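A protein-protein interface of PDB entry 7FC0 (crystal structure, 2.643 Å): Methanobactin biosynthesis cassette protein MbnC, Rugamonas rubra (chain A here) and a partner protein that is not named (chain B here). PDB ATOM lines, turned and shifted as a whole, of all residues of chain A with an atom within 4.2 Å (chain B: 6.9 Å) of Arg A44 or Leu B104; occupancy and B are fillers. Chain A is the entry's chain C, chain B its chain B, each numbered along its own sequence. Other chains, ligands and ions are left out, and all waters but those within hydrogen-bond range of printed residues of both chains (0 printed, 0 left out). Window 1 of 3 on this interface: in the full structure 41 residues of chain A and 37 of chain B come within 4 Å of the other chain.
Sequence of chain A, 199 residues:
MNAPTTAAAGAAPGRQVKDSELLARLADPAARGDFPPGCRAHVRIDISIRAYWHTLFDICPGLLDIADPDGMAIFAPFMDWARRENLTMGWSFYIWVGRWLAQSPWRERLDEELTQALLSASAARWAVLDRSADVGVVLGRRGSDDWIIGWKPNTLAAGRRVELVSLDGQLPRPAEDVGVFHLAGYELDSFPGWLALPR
Of the 19 printed residues of chain B, 11 touch a printed residue of chain A.
Printed residues of chain B that touch a printed residue of chain A: Leu B101, His B103, Leu B104, Gly B105, Glu B106, Tyr B136, Ile B139, Val B140, Ala B200, Ile B202 and Val B206.
Hydrophobic or aromatic side chains of chain B within 4 Å of the printed part of chain A: Leu B101, His B103, Tyr B136, Ile B139, Val B140, Ala B200, Ile B202 and Val B206.
Hydrophobic or aromatic side chains of chain A within 4 Å of the printed part of chain B: Leu A26, His A42, Val A43 and Ile A47.
Among the printed residues, no Asp or Glu carboxylate lies within 4 Å of a Lys or Arg side-chain nitrogen of the other chain.
NH1 of Arg A44 sits at hydrogen-bond distance from ND1 of His B103 (3.1 Å).
The backbone carbonyl oxygen of Leu B104 is in hydrogen-bond range of the guanidinium group of Arg A44.
The backbone NH (N) of Glu B106 is in hydrogen-bond range of the side-chain carboxylate (OD2) of Asp A19, 2.7 Å away.
The backbone carbonyl oxygen (O) of Ile B139 sits at hydrogen-bond distance from the guanidinium group (NH1) of Arg A40.
The backbone carbonyl oxygen (O) of Val B140 sits close to the guanidinium group (NH1) of Arg A40 (3.5 Å).
Among the printed residues, pairs that only touch across the chains: Asp A19 with Gly B105 (3.1 Å), Asp A46 with Ile B202 (3.2 Å), Val A43 with Val B206 (3.2 Å), Asp A19 with Val B140 (3.6 Å), Val A43 with Ala B200 (3.6 Å), Ile A47 with His B103 (3.7 Å), Arg A44 with Tyr B136 (3.8 Å), Arg A44 with Val B140 (3.8 Å), Ile A47 with Ala B200 (3.9 Å), Arg A44 with Gly B105 (3.9 Å), Ala A41 with Val B140 (3.9 Å), Arg A40 with Val B206 (3.9 Å), Asp A19 with Tyr B136 (3.9 Å), His A42 with Ile B202 (3.9 Å), Arg A44 with Ile B139 (3.97 Å) and Leu A26 with Leu B101 (3.998 Å).
The backbone NH (N) of Tyr B93 sits at hydrogen-bond distance from the backbone carbonyl oxygen (O) of Gly B105, at 2.8 Å.
The backbone carbonyl oxygen (O) of Phe B94 is in hydrogen-bond range of the backbone NH (N) of Leu B101.
The side-chain hydroxyl of Tyr B136 sits at hydrogen-bond distance from the backbone carbonyl oxygen of Leu B104 (2.6 Å).
The backbone NH of Ala B200 is in hydrogen-bond range of the backbone carbonyl oxygen of Val B206, at 3.3 Å.
The guanidinium group (NE) of Arg A44 is in salt-bridge range of the side-chain carboxylate (OD1) of Asp A19 (2.6 Å).
The side-chain hydroxyl (OG) of Ser A48 lies within hydrogen-bond range of the backbone carbonyl oxygen (O) of Leu A26, at 2.5 Å.
Of chain B, only His B103, Leu B104, Gly B105, Tyr B136, Ile B139 and Val B140 come within 4 Å of Arg A44.
Leu B104 touches one residue of chain A.
Of the printed residues of chain A, Glu B106 touches Asp A19.
Printed residues of chain B within 4 Å of Arg A40: Ile B139, Val B140 and Val B206.
Printed residues of chain A within 4 Å of Ile B139: Arg A40 (2.7 Å) and Arg A44 (3.97 Å).
Printed residues of chain A within 4 Å of Ala B200: Val A43 and Ile A47.
Printed residues of chain B within 4 Å of Ala A41: Val B140 (3.9 Å).
Ala B92 touches none of the printed residues of chain A.
The nearest printed residue of chain A that does not touch Leu B104 is Asp A19 (4.2 Å).
The nearest printed residue of chain B that does not touch Leu A26 is His B103 (4.3 Å).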
ATOM      1  N   ASP A  19      -6.221  -1.529 -33.050  1.00  0.00           N
ATOM      2  CA  ASP A  19      -5.696  -2.398 -31.991  1.00  0.00           C
ATOM      3  C   ASP A  19      -4.239  -2.811 -32.253  1.00  0.00           C
ATOM      4  O   ASP A  19      -3.460  -2.998 -31.306  1.00  0.00           O
ATOM      5  CB  ASP A  19      -6.594  -3.631 -31.823  1.00  0.00           C
ATOM      6  CG  ASP A  19      -6.619  -4.161 -30.375  1.00  0.00           C
ATOM      7  OD1 ASP A  19      -6.014  -3.527 -29.479  1.00  0.00           O
ATOM      8  OD2 ASP A  19      -7.226  -5.228 -30.136  1.00  0.00           O
ATOM      9  N   LEU A  26      -0.473  -3.895 -24.217  1.00  0.00           N
ATOM     10  CA  LEU A  26      -1.581  -4.641 -23.637  1.00  0.00           C
ATOM     11  C   LEU A  26      -1.208  -5.457 -22.402  1.00  0.00           C
ATOM     12  O   LEU A  26      -2.118  -5.897 -21.685  1.00  0.00           O
ATOM     13  CB  LEU A  26      -2.200  -5.549 -24.693  1.00  0.00           C
ATOM     14  CG  LEU A  26      -3.005  -4.836 -25.780  1.00  0.00           C
ATOM     15  CD1 LEU A  26      -3.825  -5.834 -26.592  1.00  0.00           C
ATOM     16  CD2 LEU A  26      -3.907  -3.781 -25.175  1.00  0.00           C
ATOM     17  N   ARG A  40     -11.815   5.665 -25.907  1.00  0.00           N
ATOM     18  CA  ARG A  40     -11.868   4.217 -26.051  1.00  0.00           C
ATOM     19  C   ARG A  40     -10.481   3.581 -26.038  1.00  0.00           C
ATOM     20  O   ARG A  40     -10.348   2.414 -25.654  1.00  0.00           O
ATOM     21  CB  ARG A  40     -12.613   3.845 -27.334  1.00  0.00           C
ATOM     22  CG  ARG A  40     -14.101   4.082 -27.264  1.00  0.00           C
ATOM     23  CD  ARG A  40     -14.764   3.767 -28.588  1.00  0.00           C
ATOM     24  NE  ARG A  40     -14.292   4.671 -29.628  1.00  0.00           N
ATOM     25  CZ  ARG A  40     -13.635   4.280 -30.717  1.00  0.00           C
ATOM     26  NH1 ARG A  40     -13.382   2.994 -30.930  1.00  0.00           N
ATOM     27  NH2 ARG A  40     -13.241   5.177 -31.609  1.00  0.00           N
ATOM     28  N   ALA A  41      -9.437   4.298 -26.474  1.00  0.00           N
ATOM     29  CA  ALA A  41      -8.105   3.696 -26.410  1.00  0.00           C
ATOM     30  C   ALA A  41      -7.694   3.421 -24.969  1.00  0.00           C
ATOM     31  O   ALA A  41      -7.139   2.357 -24.672  1.00  0.00           O
ATOM     32  CB  ALA A  41      -7.062   4.574 -27.103  1.00  0.00           C
ATOM     33  N   HIS A  42      -7.977   4.361 -24.058  1.00  0.00           N
ATOM     34  CA  HIS A  42      -7.580   4.190 -22.662  1.00  0.00           C
ATOM     35  C   HIS A  42      -8.267   2.980 -22.045  1.00  0.00           C
ATOM     36  O   HIS A  42      -7.625   2.158 -21.383  1.00  0.00           O
ATOM     37  CB  HIS A  42      -7.899   5.469 -21.871  1.00  0.00           C
ATOM     38  CG  HIS A  42      -7.691   5.352 -20.385  1.00  0.00           C
ATOM     39  ND1 HIS A  42      -6.473   5.590 -19.781  1.00  0.00           N
ATOM     40  CD2 HIS A  42      -8.551   5.048 -19.382  1.00  0.00           C
ATOM     41  CE1 HIS A  42      -6.591   5.424 -18.475  1.00  0.00           C
ATOM     42  NE2 HIS A  42      -7.840   5.091 -18.208  1.00  0.00           N
ATOM     43  N   VAL A  43      -9.583   2.867 -22.237  1.00  0.00           N
ATOM     44  CA  VAL A  43     -10.333   1.765 -21.645  1.00  0.00           C
ATOM     45  C   VAL A  43      -9.831   0.429 -22.171  1.00  0.00           C
ATOM     46  O   VAL A  43      -9.755  -0.556 -21.428  1.00  0.00           O
ATOM     47  CB  VAL A  43     -11.842   1.921 -21.889  1.00  0.00           C
ATOM     48  CG1 VAL A  43     -12.540   0.869 -21.106  1.00  0.00           C
ATOM     49  CG2 VAL A  43     -12.331   3.284 -21.447  1.00  0.00           C
ATOM     50  N   ARG A  44      -9.535   0.359 -23.473  1.00  0.00           N
ATOM     51  CA  ARG A  44      -9.092  -0.896 -24.074  1.00  0.00           C
ATOM     52  C   ARG A  44      -7.845  -1.441 -23.379  1.00  0.00           C
ATOM     53  O   ARG A  44      -7.785  -2.624 -23.030  1.00  0.00           O
ATOM     54  CB  ARG A  44      -8.845  -0.691 -25.568  1.00  0.00           C
ATOM     55  CG  ARG A  44      -8.757  -1.969 -26.371  1.00  0.00           C
ATOM     56  CD  ARG A  44      -7.321  -2.354 -26.518  1.00  0.00           C
ATOM     57  NE  ARG A  44      -7.170  -3.664 -27.136  1.00  0.00           N
ATOM     58  CZ  ARG A  44      -7.396  -4.814 -26.515  1.00  0.00           C
ATOM     59  NH1 ARG A  44      -7.785  -4.825 -25.248  1.00  0.00           N
ATOM     60  NH2 ARG A  44      -7.220  -5.954 -27.160  1.00  0.00           N
ATOM     61  N   ILE A  45      -6.829  -0.599 -23.194  1.00  0.00           N
ATOM     62  CA  ILE A  45      -5.640  -1.011 -22.448  1.00  0.00           C
ATOM     63  C   ILE A  45      -6.021  -1.529 -21.070  1.00  0.00           C
ATOM     64  O   ILE A  45      -5.553  -2.589 -20.645  1.00  0.00           O
ATOM     65  CB  ILE A  45      -4.643   0.149 -22.340  1.00  0.00           C
ATOM     66  CG1 ILE A  45      -4.300   0.660 -23.742  1.00  0.00           C
ATOM     67  CG2 ILE A  45      -3.417  -0.328 -21.612  1.00  0.00           C
ATOM     68  CD1 ILE A  45      -3.047   1.507 -23.832  1.00  0.00           C
ATOM     69  N   ASP A  46      -6.881  -0.782 -20.350  1.00  0.00           N
ATOM     70  CA  ASP A  46      -7.297  -1.165 -19.000  1.00  0.00           C
ATOM     71  C   ASP A  46      -8.021  -2.500 -18.998  1.00  0.00           C
ATOM     72  O   ASP A  46      -7.759  -3.358 -18.149  1.00  0.00           O
ATOM     73  CB  ASP A  46      -8.203  -0.093 -18.397  1.00  0.00           C
ATOM     74  CG  ASP A  46      -8.593  -0.406 -16.940  1.00  0.00           C
ATOM     75  OD1 ASP A  46      -7.770  -0.120 -16.036  1.00  0.00           O
ATOM     76  OD2 ASP A  46      -9.708  -0.943 -16.702  1.00  0.00           O
ATOM     77  N   ILE A  47      -8.979  -2.670 -19.918  1.00  0.00           N
ATOM     78  CA  ILE A  47      -9.698  -3.934 -20.070  1.00  0.00           C
ATOM     79  C   ILE A  47      -8.732  -5.100 -20.070  1.00  0.00           C
ATOM     80  O   ILE A  47      -8.996  -6.148 -19.463  1.00  0.00           O
ATOM     81  CB  ILE A  47     -10.549  -3.903 -21.349  1.00  0.00           C
ATOM     82  CG1 ILE A  47     -11.665  -2.887 -21.160  1.00  0.00           C
ATOM     83  CG2 ILE A  47     -11.084  -5.297 -21.693  1.00  0.00           C
ATOM     84  CD1 ILE A  47     -12.637  -2.839 -22.255  1.00  0.00           C
ATOM     85  N   SER A  48      -7.571  -4.913 -20.705  1.00  0.00           N
ATOM     86  CA  SER A  48      -6.612  -5.991 -20.849  1.00  0.00           C
ATOM     87  C   SER A  48      -5.714  -6.116 -19.616  1.00  0.00           C
ATOM     88  O   SER A  48      -5.450  -7.231 -19.158  1.00  0.00           O
ATOM     89  CB  SER A  48      -5.814  -5.746 -22.136  1.00  0.00           C
ATOM     90  OG  SER A  48      -4.543  -6.338 -22.130  1.00  0.00           O
ATOM     91  N   MET B  56     -11.603 -22.599 -30.408  1.00  0.00           N
ATOM     92  CA  MET B  56     -11.037 -21.438 -29.742  1.00  0.00           C
ATOM     93  C   MET B  56      -9.579 -21.176 -30.089  1.00  0.00           C
ATOM     94  O   MET B  56      -9.238 -20.046 -30.430  1.00  0.00           O
ATOM     95  CB  MET B  56     -11.173 -21.596 -28.220  1.00  0.00           C
ATOM     96  CG  MET B  56     -10.664 -20.411 -27.432  1.00  0.00           C
ATOM     97  SD  MET B  56     -11.775 -19.020 -27.582  1.00  0.00           S
ATOM     98  CE  MET B  56     -10.933 -17.938 -28.735  1.00  0.00           C
ATOM     99  N   PHE B  57      -8.723 -22.188 -30.100  1.00  0.00           N
ATOM    100  CA  PHE B  57      -7.285 -21.945 -30.147  1.00  0.00           C
ATOM    101  C   PHE B  57      -6.599 -22.661 -31.300  1.00  0.00           C
ATOM    102  O   PHE B  57      -5.521 -23.235 -31.132  1.00  0.00           O
ATOM    103  CB  PHE B  57      -6.633 -22.347 -28.834  1.00  0.00           C
ATOM    104  CG  PHE B  57      -6.942 -21.431 -27.703  1.00  0.00           C
ATOM    105  CD1 PHE B  57      -6.488 -20.120 -27.708  1.00  0.00           C
ATOM    106  CD2 PHE B  57      -7.664 -21.885 -26.603  1.00  0.00           C
ATOM    107  CE1 PHE B  57      -6.760 -19.263 -26.629  1.00  0.00           C
ATOM    108  CE2 PHE B  57      -7.932 -21.043 -25.525  1.00  0.00           C
ATOM    109  CZ  PHE B  57      -7.483 -19.732 -25.537  1.00  0.00           C
ATOM    110  N   HIS B  90     -12.023 -18.282 -35.107  1.00  0.00           N
ATOM    111  CA  HIS B  90     -11.836 -16.873 -34.762  1.00  0.00           C
ATOM    112  C   HIS B  90     -10.790 -16.180 -35.619  1.00  0.00           C
ATOM    113  O   HIS B  90      -9.799 -16.783 -36.024  1.00  0.00           O
ATOM    114  CB  HIS B  90     -11.393 -16.717 -33.316  1.00  0.00           C
ATOM    115  CG  HIS B  90     -12.424 -17.136 -32.330  1.00  0.00           C
ATOM    116  ND1 HIS B  90     -12.572 -18.442 -31.932  1.00  0.00           N
ATOM    117  CD2 HIS B  90     -13.364 -16.429 -31.672  1.00  0.00           C
ATOM    118  CE1 HIS B  90     -13.561 -18.524 -31.065  1.00  0.00           C
ATOM    119  NE2 HIS B  90     -14.056 -17.316 -30.888  1.00  0.00           N
ATOM    120  N   ALA B  92      -8.389 -13.109 -34.821  1.00  0.00           N
ATOM    121  CA  ALA B  92      -7.913 -12.225 -33.768  1.00  0.00           C
ATOM    122  C   ALA B  92      -6.422 -12.484 -33.570  1.00  0.00           C
ATOM    123  O   ALA B  92      -5.919 -13.558 -33.899  1.00  0.00           O
ATOM    124  CB  ALA B  92      -8.682 -12.451 -32.464  1.00  0.00           C
ATOM    125  N   TYR B  93      -5.732 -11.502 -32.984  1.00  0.00           N
ATOM    126  CA  TYR B  93      -4.365 -11.701 -32.524  1.00  0.00           C
ATOM    127  C   TYR B  93      -4.393 -12.422 -31.184  1.00  0.00           C
ATOM    128  O   TYR B  93      -5.133 -12.027 -30.275  1.00  0.00           O
ATOM    129  CB  TYR B  93      -3.650 -10.370 -32.357  1.00  0.00           C
ATOM    130  CG  TYR B  93      -3.464  -9.577 -33.599  1.00  0.00           C
ATOM    131  CD1 TYR B  93      -2.829 -10.120 -34.713  1.00  0.00           C
ATOM    132  CD2 TYR B  93      -3.899  -8.267 -33.663  1.00  0.00           C
ATOM    133  CE1 TYR B  93      -2.658  -9.376 -35.866  1.00  0.00           C
ATOM    134  CE2 TYR B  93      -3.715  -7.515 -34.798  1.00  0.00           C
ATOM    135  CZ  TYR B  93      -3.105  -8.082 -35.904  1.00  0.00           C
ATOM    136  OH  TYR B  93      -2.940  -7.341 -37.044  1.00  0.00           O
ATOM    137  N   PHE B  94      -3.584 -13.470 -31.055  1.00  0.00           N
ATOM    138  CA  PHE B  94      -3.488 -14.201 -29.799  1.00  0.00           C
ATOM    139  C   PHE B  94      -2.214 -13.877 -29.049  1.00  0.00           C
ATOM    140  O   PHE B  94      -2.106 -14.211 -27.868  1.00  0.00           O
ATOM    141  CB  PHE B  94      -3.556 -15.722 -30.034  1.00  0.00           C
ATOM    142  CG  PHE B  94      -4.923 -16.212 -30.395  1.00  0.00           C
ATOM    143  CD1 PHE B  94      -5.379 -16.124 -31.719  1.00  0.00           C
ATOM    144  CD2 PHE B  94      -5.780 -16.715 -29.426  1.00  0.00           C
ATOM    145  CE1 PHE B  94      -6.637 -16.531 -32.068  1.00  0.00           C
ATOM    146  CE2 PHE B  94      -7.057 -17.152 -29.783  1.00  0.00           C
ATOM    147  CZ  PHE B  94      -7.475 -17.068 -31.121  1.00  0.00           C
ATOM    148  N   SER B  95      -1.269 -13.216 -29.701  1.00  0.00           N
ATOM    149  CA  SER B  95       0.024 -12.964 -29.110  1.00  0.00           C
ATOM    150  C   SER B  95       0.656 -11.782 -29.820  1.00  0.00           C
ATOM    151  O   SER B  95       0.264 -11.419 -30.929  1.00  0.00           O
ATOM    152  CB  SER B  95       0.910 -14.201 -29.213  1.00  0.00           C
ATOM    153  OG  SER B  95       1.365 -14.328 -30.537  1.00  0.00           O
ATOM    154  N   LEU B 101      -1.612 -12.633 -25.485  1.00  0.00           N
ATOM    155  CA  LEU B 101      -2.593 -11.612 -25.151  1.00  0.00           C
ATOM    156  C   LEU B 101      -3.738 -12.277 -24.399  1.00  0.00           C
ATOM    157  O   LEU B 101      -4.470 -13.087 -24.976  1.00  0.00           O
ATOM    158  CB  LEU B 101      -3.128 -10.928 -26.402  1.00  0.00           C
ATOM    159  CG  LEU B 101      -2.044 -10.233 -27.209  1.00  0.00           C
ATOM    160  CD1 LEU B 101      -2.633  -9.789 -28.574  1.00  0.00           C
ATOM    161  CD2 LEU B 101      -1.484  -9.077 -26.431  1.00  0.00           C
ATOM    162  N   TYR B 102      -3.912 -11.909 -23.126  1.00  0.00           N
ATOM    163  CA  TYR B 102      -4.993 -12.479 -22.338  1.00  0.00           C
ATOM    164  C   TYR B 102      -6.347 -11.912 -22.738  1.00  0.00           C
ATOM    165  O   TYR B 102      -7.376 -12.521 -22.444  1.00  0.00           O
ATOM    166  CB  TYR B 102      -4.753 -12.226 -20.853  1.00  0.00           C
ATOM    167  CG  TYR B 102      -3.688 -13.096 -20.246  1.00  0.00           C
ATOM    168  CD1 TYR B 102      -2.839 -13.856 -21.043  1.00  0.00           C
ATOM    169  CD2 TYR B 102      -3.539 -13.167 -18.868  1.00  0.00           C
ATOM    170  CE1 TYR B 102      -1.867 -14.657 -20.484  1.00  0.00           C
ATOM    171  CE2 TYR B 102      -2.578 -13.960 -18.302  1.00  0.00           C
ATOM    172  CZ  TYR B 102      -1.737 -14.706 -19.112  1.00  0.00           C
ATOM    173  OH  TYR B 102      -0.760 -15.508 -18.557  1.00  0.00           O
ATOM    174  N   HIS B 103      -6.373 -10.750 -23.374  1.00  0.00           N
ATOM    175  CA  HIS B 103      -7.572 -10.214 -23.999  1.00  0.00           C
ATOM    176  C   HIS B 103      -7.239 -10.036 -25.467  1.00  0.00           C
ATOM    177  O   HIS B 103      -6.387  -9.211 -25.812  1.00  0.00           O
ATOM    178  CB  HIS B 103      -7.995  -8.891 -23.370  1.00  0.00           C
ATOM    179  CG  HIS B 103      -9.277  -8.359 -23.921  1.00  0.00           C
ATOM    180  ND1 HIS B 103      -9.321  -7.494 -24.993  1.00  0.00           N
ATOM    181  CD2 HIS B 103     -10.564  -8.578 -23.559  1.00  0.00           C
ATOM    182  CE1 HIS B 103     -10.581  -7.204 -25.271  1.00  0.00           C
ATOM    183  NE2 HIS B 103     -11.353  -7.848 -24.414  1.00  0.00           N
ATOM    184  N   LEU B 104      -7.893 -10.820 -26.320  1.00  0.00           N
ATOM    185  CA  LEU B 104      -7.460 -10.973 -27.707  1.00  0.00           C
ATOM    186  C   LEU B 104      -7.460  -9.631 -28.433  1.00  0.00           C
ATOM    187  O   LEU B 104      -8.210  -8.716 -28.087  1.00  0.00           O
ATOM    188  CB  LEU B 104      -8.339 -11.995 -28.425  1.00  0.00           C
ATOM    189  CG  LEU B 104      -8.373 -13.377 -27.744  1.00  0.00           C
ATOM    190  CD1 LEU B 104      -8.876 -14.469 -28.640  1.00  0.00           C
ATOM    191  CD2 LEU B 104      -7.009 -13.780 -27.243  1.00  0.00           C
ATOM    192  N   GLY B 105      -6.558  -9.494 -29.410  1.00  0.00           N
ATOM    193  CA  GLY B 105      -6.428  -8.264 -30.168  1.00  0.00           C
ATOM    194  C   GLY B 105      -7.211  -8.325 -31.465  1.00  0.00           C
ATOM    195  O   GLY B 105      -7.298  -9.377 -32.107  1.00  0.00           O
ATOM    196  N   GLU B 106      -7.744  -7.168 -31.870  1.00  0.00           N
ATOM    197  CA  GLU B 106      -8.425  -7.043 -33.156  1.00  0.00           C
ATOM    198  C   GLU B 106      -7.407  -6.967 -34.303  1.00  0.00           C
ATOM    199  O   GLU B 106      -6.461  -6.173 -34.249  1.00  0.00           O
ATOM    200  CB  GLU B 106      -9.303  -5.798 -33.148  1.00  0.00           C
ATOM    201  CG  GLU B 106     -10.248  -5.706 -34.315  1.00  0.00           C
ATOM    202  CD  GLU B 106     -11.210  -4.537 -34.217  1.00  0.00           C
ATOM    203  OE1 GLU B 106     -10.801  -3.440 -33.756  1.00  0.00           O
ATOM    204  OE2 GLU B 106     -12.378  -4.724 -34.617  1.00  0.00           O
ATOM    205  N   TYR B 136     -15.274  -9.818 -34.545  1.00  0.00           N
ATOM    206  CA  TYR B 136     -14.687  -9.350 -33.290  1.00  0.00           C
ATOM    207  C   TYR B 136     -15.548  -8.259 -32.645  1.00  0.00           C
ATOM    208  O   TYR B 136     -16.091  -7.400 -33.340  1.00  0.00           O
ATOM    209  CB  TYR B 136     -13.284  -8.801 -33.540  1.00  0.00           C
ATOM    210  CG  TYR B 136     -12.483  -8.454 -32.303  1.00  0.00           C
ATOM    211  CD1 TYR B 136     -12.524  -7.170 -31.761  1.00  0.00           C
ATOM    212  CD2 TYR B 136     -11.647  -9.386 -31.709  1.00  0.00           C
ATOM    213  CE1 TYR B 136     -11.789  -6.830 -30.658  1.00  0.00           C
ATOM    214  CE2 TYR B 136     -10.899  -9.051 -30.585  1.00  0.00           C
ATOM    215  CZ  TYR B 136     -10.983  -7.767 -30.065  1.00  0.00           C
ATOM    216  OH  TYR B 136     -10.263  -7.397 -28.950  1.00  0.00           O
ATOM    217  N   ILE B 139     -13.493  -2.576 -29.955  1.00  0.00           N
ATOM    218  CA  ILE B 139     -13.464  -1.512 -28.951  1.00  0.00           C
ATOM    219  C   ILE B 139     -12.842  -0.246 -29.509  1.00  0.00           C
ATOM    220  O   ILE B 139     -13.405   0.840 -29.379  1.00  0.00           O
ATOM    221  CB  ILE B 139     -12.733  -1.981 -27.678  1.00  0.00           C
ATOM    222  CG1 ILE B 139     -13.440  -3.205 -27.095  1.00  0.00           C
ATOM    223  CG2 ILE B 139     -12.666  -0.867 -26.647  1.00  0.00           C
ATOM    224  CD1 ILE B 139     -12.536  -4.091 -26.310  1.00  0.00           C
ATOM    225  N   VAL B 140     -11.692  -0.347 -30.176  1.00  0.00           N
ATOM    226  CA  VAL B 140     -11.046   0.827 -30.760  1.00  0.00           C
ATOM    227  C   VAL B 140     -11.316   0.870 -32.264  1.00  0.00           C
ATOM    228  O   VAL B 140     -12.279   0.264 -32.743  1.00  0.00           O
ATOM    229  CB  VAL B 140      -9.545   0.874 -30.446  1.00  0.00           C
ATOM    230  CG1 VAL B 140      -9.361   1.021 -28.938  1.00  0.00           C
ATOM    231  CG2 VAL B 140      -8.863  -0.358 -30.973  1.00  0.00           C
ATOM    232  N   ALA B 200     -17.182  -2.007 -19.262  1.00  0.00           N
ATOM    233  CA  ALA B 200     -15.861  -2.131 -18.667  1.00  0.00           C
ATOM    234  C   ALA B 200     -15.902  -1.634 -17.242  1.00  0.00           C
ATOM    235  O   ALA B 200     -16.598  -0.666 -16.935  1.00  0.00           O
ATOM    236  CB  ALA B 200     -14.833  -1.333 -19.456  1.00  0.00           C
ATOM    237  N   ILE B 202     -14.036   0.190 -15.516  1.00  0.00           N
ATOM    238  CA  ILE B 202     -13.667   1.587 -15.292  1.00  0.00           C
ATOM    239  C   ILE B 202     -14.375   2.544 -16.239  1.00  0.00           C
ATOM    240  O   ILE B 202     -14.109   3.753 -16.189  1.00  0.00           O
ATOM    241  CB  ILE B 202     -12.133   1.793 -15.362  1.00  0.00           C
ATOM    242  CG1 ILE B 202     -11.590   1.613 -16.785  1.00  0.00           C
ATOM    243  CG2 ILE B 202     -11.402   0.842 -14.423  1.00  0.00           C
ATOM    244  CD1 ILE B 202     -11.262   2.900 -17.494  1.00  0.00           C
ATOM    245  N   VAL B 206     -18.063   2.044 -22.693  1.00  0.00           N
ATOM    246  CA  VAL B 206     -17.534   1.072 -23.643  1.00  0.00           C
ATOM    247  C   VAL B 206     -18.106  -0.289 -23.283  1.00  0.00           C
ATOM    248  O   VAL B 206     -18.238  -0.637 -22.103  1.00  0.00           O
ATOM    249  CB  VAL B 206     -15.995   1.020 -23.671  1.00  0.00           C
ATOM    250  CG1 VAL B 206     -15.424   2.371 -24.031  1.00  0.00           C
ATOM    251  CG2 VAL B 206     -15.501   0.595 -22.338  1.00  0.00           C
